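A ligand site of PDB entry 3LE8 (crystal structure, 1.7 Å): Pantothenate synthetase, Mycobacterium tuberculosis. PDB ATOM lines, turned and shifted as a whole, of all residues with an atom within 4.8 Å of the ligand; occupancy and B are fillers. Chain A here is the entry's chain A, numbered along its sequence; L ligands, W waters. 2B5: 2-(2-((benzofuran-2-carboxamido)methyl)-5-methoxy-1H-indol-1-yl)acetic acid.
An oxygen (O) of the ligand lies within hydrogen-bond range of a ring nitrogen (NE2) of His 44, 2.8 Å away. A ring nitrogen (NE2) of His 47 is in hydrogen-bond range of an oxygen (OAC) of the ligand. N of Met 40 lies within hydrogen-bond range of OAC of the ligand (3.0 Å). N of Ser 197 sits at hydrogen-bond distance from O of the ligand, 3.0 Å away. N of Val 187 is in hydrogen-bond range of OAQ of the ligand. An oxygen (OXT) of the ligand sits at hydrogen-bond distance from the side-chain hydroxyl of Ser 196 (3.1 Å).
A ring nitrogen (ND1) of His 47 sits at hydrogen-bond distance from the backbone NH (N) of His 44 (3.0 Å). A ring nitrogen (ND1) of His 44 lies within hydrogen-bond range of the backbone NH (N) of Gly 46 (2.9 Å). The side-chain hydroxyl of Ser 197 sits at hydrogen-bond distance from the side-chain hydroxyl of Tyr 82 (3.1 Å). OG1 of Thr 39 lies within hydrogen-bond range of N of Gly 41 (3.0 Å). O of Val 187 lies within hydrogen-bond range of N of Met 195 (3.0 Å). The backbone NH (N) of Val 184 sits at hydrogen-bond distance from the backbone carbonyl oxygen (O) of Phe 157 (2.8 Å). The side-chain hydroxyl (OG1) of Thr 186 is in hydrogen-bond range of the backbone NH (N) of Lys 160. OD1 of Asp 161 is in salt-bridge range of NZ of Lys 160 (3.9 Å).
O of Pro 38 touches CAM of the ligand, at 3.4 Å. Thr 39 touches the ligand. O of Gly 46 touches CAA of the ligand, 3.3 Å away. CD2 of Leu 50 touches CAA of the ligand, at 3.6 Å. Val 143 touches the ligand (CG2 to CAF, 3.3 Å). Phe 157 touches the ligand. CB of Lys 160 touches CAJ of the ligand, at 3.5 Å. Asp 161 touches the ligand. Gln 164 touches the ligand (NE2 to CAI, 3.5 Å). O of Val 184 touches CAA of the ligand, at 3.9 Å. O of Pro 185 touches CAA of the ligand, at 3.3 Å. Thr 186 touches the ligand. Met 195 touches the ligand. The nearest printed residue that does not touch the ligand is Gly 158 (4.02 Å).
Water W1 lies within hydrogen-bond range of OD2 of Asp 161 (2.9 Å), NAP of the ligand (2.9 Å) and NE2 of Gln 164 (3.0 Å). Water W4 lies within hydrogen-bond range of O of Gly 41 (2.6 Å), OH of Tyr 82 (2.7 Å) and OAC of the ligand (3.0 Å). Water W2 lies within hydrogen-bond range of OD2 of Asp 161 (2.8 Å) and OXT of the ligand (3.4 Å).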
ATOM      1  N   PRO A  38      -7.344 -27.985 -19.883  1.00  0.00           N
ATOM      2  CA  PRO A  38      -7.996 -26.645 -20.044  1.00  0.00           C
ATOM      3  C   PRO A  38      -9.212 -26.538 -19.177  1.00  0.00           C
ATOM      4  O   PRO A  38      -9.999 -27.506 -19.051  1.00  0.00           O
ATOM      5  CB  PRO A  38      -8.399 -26.649 -21.514  1.00  0.00           C
ATOM      6  CG  PRO A  38      -7.593 -27.811 -22.160  1.00  0.00           C
ATOM      7  CD  PRO A  38      -7.639 -28.818 -21.073  1.00  0.00           C
ATOM      8  N   THR A  39      -9.403 -25.368 -18.562  1.00  0.00           N
ATOM      9  CA  THR A  39     -10.533 -25.208 -17.649  1.00  0.00           C
ATOM     10  C   THR A  39     -11.075 -23.783 -17.794  1.00  0.00           C
ATOM     11  O   THR A  39     -10.328 -22.893 -18.215  1.00  0.00           O
ATOM     12  CB  THR A  39     -10.202 -25.449 -16.138  1.00  0.00           C
ATOM     13  OG1 THR A  39      -9.678 -24.256 -15.513  1.00  0.00           O
ATOM     14  CG2 THR A  39      -9.121 -26.650 -15.941  1.00  0.00           C
ATOM     15  N   MET A  40     -12.282 -23.602 -17.258  1.00  0.00           N
ATOM     16  CA  MET A  40     -12.805 -22.224 -17.160  1.00  0.00           C
ATOM     17  C   MET A  40     -12.891 -21.828 -15.694  1.00  0.00           C
ATOM     18  O   MET A  40     -13.698 -20.992 -15.280  1.00  0.00           O
ATOM     19  CB  MET A  40     -14.132 -22.049 -17.906  1.00  0.00           C
ATOM     20  CG  MET A  40     -13.995 -22.173 -19.423  1.00  0.00           C
ATOM     21  SD  MET A  40     -15.190 -21.095 -20.413  1.00  0.00           S
ATOM     22  CE  MET A  40     -16.768 -21.760 -19.762  1.00  0.00           C
ATOM     23  N   GLY A  41     -11.996 -22.434 -14.914  1.00  0.00           N
ATOM     24  CA  GLY A  41     -11.953 -22.087 -13.492  1.00  0.00           C
ATOM     25  C   GLY A  41     -13.136 -22.691 -12.733  1.00  0.00           C
ATOM     26  O   GLY A  41     -13.859 -23.584 -13.218  1.00  0.00           O
ATOM     27  N   HIS A  44     -13.653 -28.002  -9.555  1.00  0.00           N
ATOM     28  CA  HIS A  44     -14.253 -28.986  -8.690  1.00  0.00           C
ATOM     29  C   HIS A  44     -13.530 -30.328  -8.873  1.00  0.00           C
ATOM     30  O   HIS A  44     -12.523 -30.428  -9.604  1.00  0.00           O
ATOM     31  CB  HIS A  44     -15.753 -29.078  -8.997  1.00  0.00           C
ATOM     32  CG  HIS A  44     -16.037 -29.299 -10.442  1.00  0.00           C
ATOM     33  ND1 HIS A  44     -15.688 -30.461 -11.098  1.00  0.00           N
ATOM     34  CD2 HIS A  44     -16.568 -28.472 -11.372  1.00  0.00           C
ATOM     35  CE1 HIS A  44     -16.041 -30.350 -12.374  1.00  0.00           C
ATOM     36  NE2 HIS A  44     -16.579 -29.159 -12.562  1.00  0.00           N
ATOM     37  N   GLY A  46     -14.158 -32.850 -10.447  1.00  0.00           N
ATOM     38  CA  GLY A  46     -14.063 -33.382 -11.809  1.00  0.00           C
ATOM     39  C   GLY A  46     -12.794 -32.820 -12.488  1.00  0.00           C
ATOM     40  O   GLY A  46     -12.024 -33.557 -13.121  1.00  0.00           O
ATOM     41  N   HIS A  47     -12.565 -31.510 -12.340  1.00  0.00           N
ATOM     42  CA  HIS A  47     -11.285 -30.966 -12.778  1.00  0.00           C
ATOM     43  C   HIS A  47     -10.077 -31.645 -12.110  1.00  0.00           C
ATOM     44  O   HIS A  47      -9.069 -31.847 -12.766  1.00  0.00           O
ATOM     45  CB  HIS A  47     -11.130 -29.457 -12.551  1.00  0.00           C
ATOM     46  CG  HIS A  47     -12.154 -28.652 -13.230  1.00  0.00           C
ATOM     47  ND1 HIS A  47     -13.246 -28.124 -12.544  1.00  0.00           N
ATOM     48  CD2 HIS A  47     -12.263 -28.244 -14.521  1.00  0.00           C
ATOM     49  CE1 HIS A  47     -13.986 -27.439 -13.394  1.00  0.00           C
ATOM     50  NE2 HIS A  47     -13.423 -27.499 -14.594  1.00  0.00           N
ATOM     51  N   ALA A  49      -9.815 -34.632 -11.103  1.00  0.00           N
ATOM     52  CA  ALA A  49      -9.602 -35.927 -11.799  1.00  0.00           C
ATOM     53  C   ALA A  49      -8.790 -35.760 -13.086  1.00  0.00           C
ATOM     54  O   ALA A  49      -7.985 -36.652 -13.452  1.00  0.00           O
ATOM     55  CB  ALA A  49     -10.924 -36.709 -12.074  1.00  0.00           C
ATOM     56  N   LEU A  50      -9.018 -34.663 -13.828  1.00  0.00           N
ATOM     57  CA  LEU A  50      -8.247 -34.457 -15.036  1.00  0.00           C
ATOM     58  C   LEU A  50      -6.792 -34.222 -14.638  1.00  0.00           C
ATOM     59  O   LEU A  50      -5.855 -34.748 -15.303  1.00  0.00           O
ATOM     60  CB  LEU A  50      -8.746 -33.223 -15.820  1.00  0.00           C
ATOM     61  CG  LEU A  50     -10.231 -33.172 -16.122  1.00  0.00           C
ATOM     62  CD1 LEU A  50     -10.574 -32.001 -17.075  1.00  0.00           C
ATOM     63  CD2 LEU A  50     -10.727 -34.484 -16.783  1.00  0.00           C
ATOM     64  N   TYR A  82     -20.940 -16.504 -15.204  1.00  0.00           N
ATOM     65  CA  TYR A  82     -20.128 -17.690 -14.963  1.00  0.00           C
ATOM     66  C   TYR A  82     -19.351 -17.578 -13.665  1.00  0.00           C
ATOM     67  O   TYR A  82     -18.744 -16.535 -13.448  1.00  0.00           O
ATOM     68  CB  TYR A  82     -19.135 -17.824 -16.074  1.00  0.00           C
ATOM     69  CG  TYR A  82     -18.716 -19.261 -16.133  1.00  0.00           C
ATOM     70  CD1 TYR A  82     -19.540 -20.212 -16.679  1.00  0.00           C
ATOM     71  CD2 TYR A  82     -17.526 -19.666 -15.552  1.00  0.00           C
ATOM     72  CE1 TYR A  82     -19.153 -21.601 -16.744  1.00  0.00           C
ATOM     73  CE2 TYR A  82     -17.145 -21.022 -15.597  1.00  0.00           C
ATOM     74  CZ  TYR A  82     -17.996 -21.977 -16.180  1.00  0.00           C
ATOM     75  OH  TYR A  82     -17.569 -23.315 -16.192  1.00  0.00           O
ATOM     76  N   VAL A 139     -15.629 -22.451 -28.608  1.00  0.00           N
ATOM     77  CA  VAL A 139     -14.857 -23.478 -27.907  1.00  0.00           C
ATOM     78  C   VAL A 139     -13.638 -23.976 -28.709  1.00  0.00           C
ATOM     79  O   VAL A 139     -12.530 -24.008 -28.226  1.00  0.00           O
ATOM     80  CB  VAL A 139     -15.729 -24.699 -27.569  1.00  0.00           C
ATOM     81  CG1 VAL A 139     -14.800 -25.759 -26.944  1.00  0.00           C
ATOM     82  CG2 VAL A 139     -16.899 -24.311 -26.607  1.00  0.00           C
ATOM     83  N   VAL A 142     -10.840 -21.351 -29.050  1.00  0.00           N
ATOM     84  CA  VAL A 142     -10.006 -21.259 -27.884  1.00  0.00           C
ATOM     85  C   VAL A 142      -9.107 -22.494 -27.659  1.00  0.00           C
ATOM     86  O   VAL A 142      -7.965 -22.331 -27.233  1.00  0.00           O
ATOM     87  CB  VAL A 142     -10.726 -20.782 -26.594  1.00  0.00           C
ATOM     88  CG1 VAL A 142     -11.488 -21.911 -25.886  1.00  0.00           C
ATOM     89  CG2 VAL A 142      -9.745 -20.035 -25.638  1.00  0.00           C
ATOM     90  N   VAL A 143      -9.629 -23.672 -27.936  1.00  0.00           N
ATOM     91  CA  VAL A 143      -8.905 -24.883 -27.671  1.00  0.00           C
ATOM     92  C   VAL A 143      -7.729 -24.918 -28.640  1.00  0.00           C
ATOM     93  O   VAL A 143      -6.576 -25.250 -28.262  1.00  0.00           O
ATOM     94  CB  VAL A 143      -9.751 -26.144 -27.872  1.00  0.00           C
ATOM     95  CG1 VAL A 143      -8.811 -27.448 -27.954  1.00  0.00           C
ATOM     96  CG2 VAL A 143     -10.810 -26.284 -26.755  1.00  0.00           C
ATOM     97  N   LEU A 146      -5.062 -22.527 -27.285  1.00  0.00           N
ATOM     98  CA  LEU A 146      -4.412 -23.031 -26.043  1.00  0.00           C
ATOM     99  C   LEU A 146      -3.440 -24.143 -26.463  1.00  0.00           C
ATOM    100  O   LEU A 146      -2.297 -24.248 -25.935  1.00  0.00           O
ATOM    101  CB  LEU A 146      -5.433 -23.653 -25.114  1.00  0.00           C
ATOM    102  CG  LEU A 146      -6.318 -22.533 -24.498  1.00  0.00           C
ATOM    103  CD1 LEU A 146      -7.313 -23.212 -23.594  1.00  0.00           C
ATOM    104  CD2 LEU A 146      -5.503 -21.646 -23.539  1.00  0.00           C
ATOM    105  N   PHE A 157      -9.754 -33.851 -21.175  1.00  0.00           N
ATOM    106  CA  PHE A 157     -11.103 -33.295 -21.061  1.00  0.00           C
ATOM    107  C   PHE A 157     -12.019 -34.325 -20.379  1.00  0.00           C
ATOM    108  O   PHE A 157     -11.828 -35.569 -20.555  1.00  0.00           O
ATOM    109  CB  PHE A 157     -11.700 -33.066 -22.475  1.00  0.00           C
ATOM    110  CG  PHE A 157     -10.972 -31.978 -23.220  1.00  0.00           C
ATOM    111  CD1 PHE A 157     -11.225 -30.675 -22.932  1.00  0.00           C
ATOM    112  CD2 PHE A 157     -10.020 -32.287 -24.183  1.00  0.00           C
ATOM    113  CE1 PHE A 157     -10.547 -29.628 -23.620  1.00  0.00           C
ATOM    114  CE2 PHE A 157      -9.348 -31.305 -24.854  1.00  0.00           C
ATOM    115  CZ  PHE A 157      -9.592 -29.976 -24.598  1.00  0.00           C
ATOM    116  N   GLY A 158     -13.040 -33.842 -19.643  1.00  0.00           N
ATOM    117  CA  GLY A 158     -14.028 -34.712 -19.019  1.00  0.00           C
ATOM    118  C   GLY A 158     -14.971 -35.226 -20.083  1.00  0.00           C
ATOM    119  O   GLY A 158     -15.229 -34.580 -21.080  1.00  0.00           O
ATOM    120  N   LYS A 160     -18.127 -35.344 -19.471  1.00  0.00           N
ATOM    121  CA  LYS A 160     -19.410 -34.789 -19.098  1.00  0.00           C
ATOM    122  C   LYS A 160     -19.939 -33.916 -20.279  1.00  0.00           C
ATOM    123  O   LYS A 160     -21.099 -34.021 -20.709  1.00  0.00           O
ATOM    124  CB  LYS A 160     -19.110 -33.988 -17.792  1.00  0.00           C
ATOM    125  CG  LYS A 160     -20.012 -32.952 -17.414  1.00  0.00           C
ATOM    126  CD  LYS A 160     -21.385 -33.421 -17.208  1.00  0.00           C
ATOM    127  CE  LYS A 160     -22.093 -32.281 -16.586  1.00  0.00           C
ATOM    128  NZ  LYS A 160     -22.303 -31.275 -17.662  1.00  0.00           N
ATOM    129  N   ASP A 161     -19.058 -33.115 -20.845  1.00  0.00           N
ATOM    130  CA  ASP A 161     -19.379 -32.340 -22.021  1.00  0.00           C
ATOM    131  C   ASP A 161     -18.940 -33.152 -23.245  1.00  0.00           C
ATOM    132  O   ASP A 161     -17.937 -32.864 -23.890  1.00  0.00           O
ATOM    133  CB  ASP A 161     -18.723 -30.987 -21.963  1.00  0.00           C
ATOM    134  CG  ASP A 161     -19.293 -30.135 -20.811  1.00  0.00           C
ATOM    135  OD1 ASP A 161     -20.484 -29.806 -20.816  1.00  0.00           O
ATOM    136  OD2 ASP A 161     -18.530 -29.872 -19.895  1.00  0.00           O
ATOM    137  N   GLN A 164     -18.819 -31.598 -26.777  1.00  0.00           N
ATOM    138  CA  GLN A 164     -17.611 -30.853 -26.855  1.00  0.00           C
ATOM    139  C   GLN A 164     -16.336 -31.739 -27.109  1.00  0.00           C
ATOM    140  O   GLN A 164     -15.500 -31.400 -27.918  1.00  0.00           O
ATOM    141  CB  GLN A 164     -17.470 -30.006 -25.577  1.00  0.00           C
ATOM    142  CG  GLN A 164     -16.214 -29.197 -25.564  1.00  0.00           C
ATOM    143  CD  GLN A 164     -16.049 -28.523 -24.203  1.00  0.00           C
ATOM    144  OE1 GLN A 164     -16.604 -27.477 -24.001  1.00  0.00           O
ATOM    145  NE2 GLN A 164     -15.385 -29.222 -23.241  1.00  0.00           N
ATOM    146  N   ILE A 168     -13.822 -31.689 -30.217  1.00  0.00           N
ATOM    147  CA  ILE A 168     -12.392 -31.493 -30.020  1.00  0.00           C
ATOM    148  C   ILE A 168     -11.575 -32.581 -30.703  1.00  0.00           C
ATOM    149  O   ILE A 168     -10.548 -32.292 -31.333  1.00  0.00           O
ATOM    150  CB  ILE A 168     -12.058 -31.315 -28.519  1.00  0.00           C
ATOM    151  CG1 ILE A 168     -12.491 -29.920 -28.108  1.00  0.00           C
ATOM    152  CG2 ILE A 168     -10.520 -31.424 -28.313  1.00  0.00           C
ATOM    153  CD1 ILE A 168     -12.597 -29.737 -26.566  1.00  0.00           C
ATOM    154  N   VAL A 184     -11.626 -38.298 -19.904  1.00  0.00           N
ATOM    155  CA  VAL A 184     -11.662 -38.810 -18.531  1.00  0.00           C
ATOM    156  C   VAL A 184     -13.075 -38.980 -18.011  1.00  0.00           C
ATOM    157  O   VAL A 184     -13.892 -38.107 -18.195  1.00  0.00           O
ATOM    158  CB  VAL A 184     -10.858 -37.875 -17.585  1.00  0.00           C
ATOM    159  CG1 VAL A 184     -10.873 -38.381 -16.125  1.00  0.00           C
ATOM    160  CG2 VAL A 184      -9.444 -37.685 -18.080  1.00  0.00           C
ATOM    161  N   PRO A 185     -13.425 -40.151 -17.459  1.00  0.00           N
ATOM    162  CA  PRO A 185     -14.845 -40.393 -17.139  1.00  0.00           C
ATOM    163  C   PRO A 185     -15.378 -39.372 -16.129  1.00  0.00           C
ATOM    164  O   PRO A 185     -14.626 -38.918 -15.264  1.00  0.00           O
ATOM    165  CB  PRO A 185     -14.862 -41.827 -16.554  1.00  0.00           C
ATOM    166  CG  PRO A 185     -13.663 -42.535 -17.294  1.00  0.00           C
ATOM    167  CD  PRO A 185     -12.592 -41.398 -17.423  1.00  0.00           C
ATOM    168  N   THR A 186     -16.643 -39.009 -16.287  1.00  0.00           N
ATOM    169  CA  THR A 186     -17.229 -37.951 -15.464  1.00  0.00           C
ATOM    170  C   THR A 186     -17.165 -38.305 -13.954  1.00  0.00           C
ATOM    171  O   THR A 186     -17.511 -39.444 -13.547  1.00  0.00           O
ATOM    172  CB  THR A 186     -18.679 -37.829 -15.898  1.00  0.00           C
ATOM    173  OG1 THR A 186     -18.686 -37.538 -17.304  1.00  0.00           O
ATOM    174  CG2 THR A 186     -19.394 -36.769 -15.162  1.00  0.00           C
ATOM    175  N   VAL A 187     -16.761 -37.341 -13.157  1.00  0.00           N
ATOM    176  CA  VAL A 187     -16.800 -37.530 -11.696  1.00  0.00           C
ATOM    177  C   VAL A 187     -18.204 -37.151 -11.219  1.00  0.00           C
ATOM    178  O   VAL A 187     -18.810 -36.223 -11.751  1.00  0.00           O
ATOM    179  CB  VAL A 187     -15.745 -36.619 -10.954  1.00  0.00           C
ATOM    180  CG1 VAL A 187     -15.893 -36.856  -9.460  1.00  0.00           C
ATOM    181  CG2 VAL A 187     -14.339 -36.961 -11.381  1.00  0.00           C
ATOM    182  N   MET A 195     -20.639 -33.883 -11.680  1.00  0.00           N
ATOM    183  CA  MET A 195     -19.897 -32.665 -11.264  1.00  0.00           C
ATOM    184  C   MET A 195     -20.194 -31.579 -12.232  1.00  0.00           C
ATOM    185  O   MET A 195     -20.103 -31.861 -13.376  1.00  0.00           O
ATOM    186  CB  MET A 195     -18.333 -32.854 -11.216  1.00  0.00           C
ATOM    187  CG  MET A 195     -17.838 -33.531  -9.871  1.00  0.00           C
ATOM    188  SD  MET A 195     -18.938 -33.110  -8.378  1.00  0.00           S
ATOM    189  CE  MET A 195     -18.133 -31.647  -7.852  1.00  0.00           C
ATOM    190  N   SER A 196     -20.383 -30.352 -11.800  1.00  0.00           N
ATOM    191  CA  SER A 196     -20.498 -29.245 -12.727  1.00  0.00           C
ATOM    192  C   SER A 196     -20.355 -27.950 -11.920  1.00  0.00           C
ATOM    193  O   SER A 196     -20.851 -27.859 -10.764  1.00  0.00           O
ATOM    194  CB  SER A 196     -21.896 -29.256 -13.357  1.00  0.00           C
ATOM    195  OG  SER A 196     -22.185 -28.044 -14.035  1.00  0.00           O
ATOM    196  N   SER A 197     -19.687 -26.982 -12.544  1.00  0.00           N
ATOM    197  CA  SER A 197     -19.621 -25.611 -12.026  1.00  0.00           C
ATOM    198  C   SER A 197     -21.021 -25.044 -11.788  1.00  0.00           C
ATOM    199  O   SER A 197     -21.189 -24.086 -11.002  1.00  0.00           O
ATOM    200  CB  SER A 197     -18.916 -24.686 -13.031  1.00  0.00           C
ATOM    201  OG  SER A 197     -19.524 -24.773 -14.323  1.00  0.00           O
HETATM  202  C   2B5 L   1     -18.647 -28.510 -15.606  1.00  0.00           C
HETATM  203  N   2B5 L   1     -16.867 -30.386 -16.053  1.00  0.00           N
HETATM  204  O   2B5 L   1     -17.927 -28.021 -14.800  1.00  0.00           O
HETATM  205  CA  2B5 L   1     -18.291 -29.865 -16.111  1.00  0.00           C
HETATM  206  CAA 2B5 L   1     -13.640 -35.752 -15.059  1.00  0.00           C
HETATM  207  OAC 2B5 L   1     -13.863 -26.141 -17.152  1.00  0.00           O
HETATM  208  CAE 2B5 L   1     -11.362 -24.931 -22.959  1.00  0.00           C
HETATM  209  CAF 2B5 L   1     -11.867 -26.078 -23.619  1.00  0.00           C
HETATM  210  CAG 2B5 L   1     -16.779 -33.854 -14.710  1.00  0.00           C
HETATM  211  CAH 2B5 L   1     -11.646 -24.760 -21.600  1.00  0.00           C
HETATM  212  CAI 2B5 L   1     -12.660 -26.975 -22.904  1.00  0.00           C
HETATM  213  CAJ 2B5 L   1     -17.364 -32.638 -15.081  1.00  0.00           C
HETATM  214  CAK 2B5 L   1     -14.636 -33.030 -15.415  1.00  0.00           C
HETATM  215  CAL 2B5 L   1     -14.686 -30.682 -16.286  1.00  0.00           C
HETATM  216  CAM 2B5 L   1     -12.780 -25.648 -19.664  1.00  0.00           C
HETATM  217  CAN 2B5 L   1     -15.700 -28.392 -16.988  1.00  0.00           C
HETATM  218  NAP 2B5 L   1     -14.886 -28.017 -18.143  1.00  0.00           N
HETATM  219  OAQ 2B5 L   1     -14.908 -35.332 -14.523  1.00  0.00           O
HETATM  220  OAR 2B5 L   1     -13.708 -27.547 -20.579  1.00  0.00           O
HETATM  221  CAT 2B5 L   1     -14.064 -26.938 -18.105  1.00  0.00           C
HETATM  222  CAU 2B5 L   1     -15.411 -34.087 -14.881  1.00  0.00           C
HETATM  223  CAV 2B5 L   1     -15.728 -29.814 -16.479  1.00  0.00           C
HETATM  224  CAW 2B5 L   1     -13.516 -26.705 -19.331  1.00  0.00           C
HETATM  225  CAX 2B5 L   1     -12.403 -25.662 -20.958  1.00  0.00           C
HETATM  226  CAY 2B5 L   1     -15.231 -31.836 -15.768  1.00  0.00           C
HETATM  227  CAZ 2B5 L   1     -12.883 -26.762 -21.594  1.00  0.00           C
HETATM  228  CBA 2B5 L   1     -16.563 -31.642 -15.612  1.00  0.00           C
HETATM  229  OXT 2B5 L   1     -19.733 -28.039 -16.009  1.00  0.00           O
HETATM  230  O   HOH W   1     -15.689 -29.778 -20.261  1.00  0.00           O
HETATM  231  O   HOH W   2     -18.451 -27.162 -19.053  1.00  0.00           O
HETATM  232  O   HOH W   3     -10.853 -21.421 -21.795  1.00  0.00           O
HETATM  233  O   HOH W   4     -15.345 -24.537 -15.150  1.00  0.00           O
HETATM  234  O   HOH W   5     -13.395 -22.392 -22.882  1.00  0.00           O
HETATM  235  O   HOH W   6     -15.544 -25.121 -22.713  1.00  0.00           O
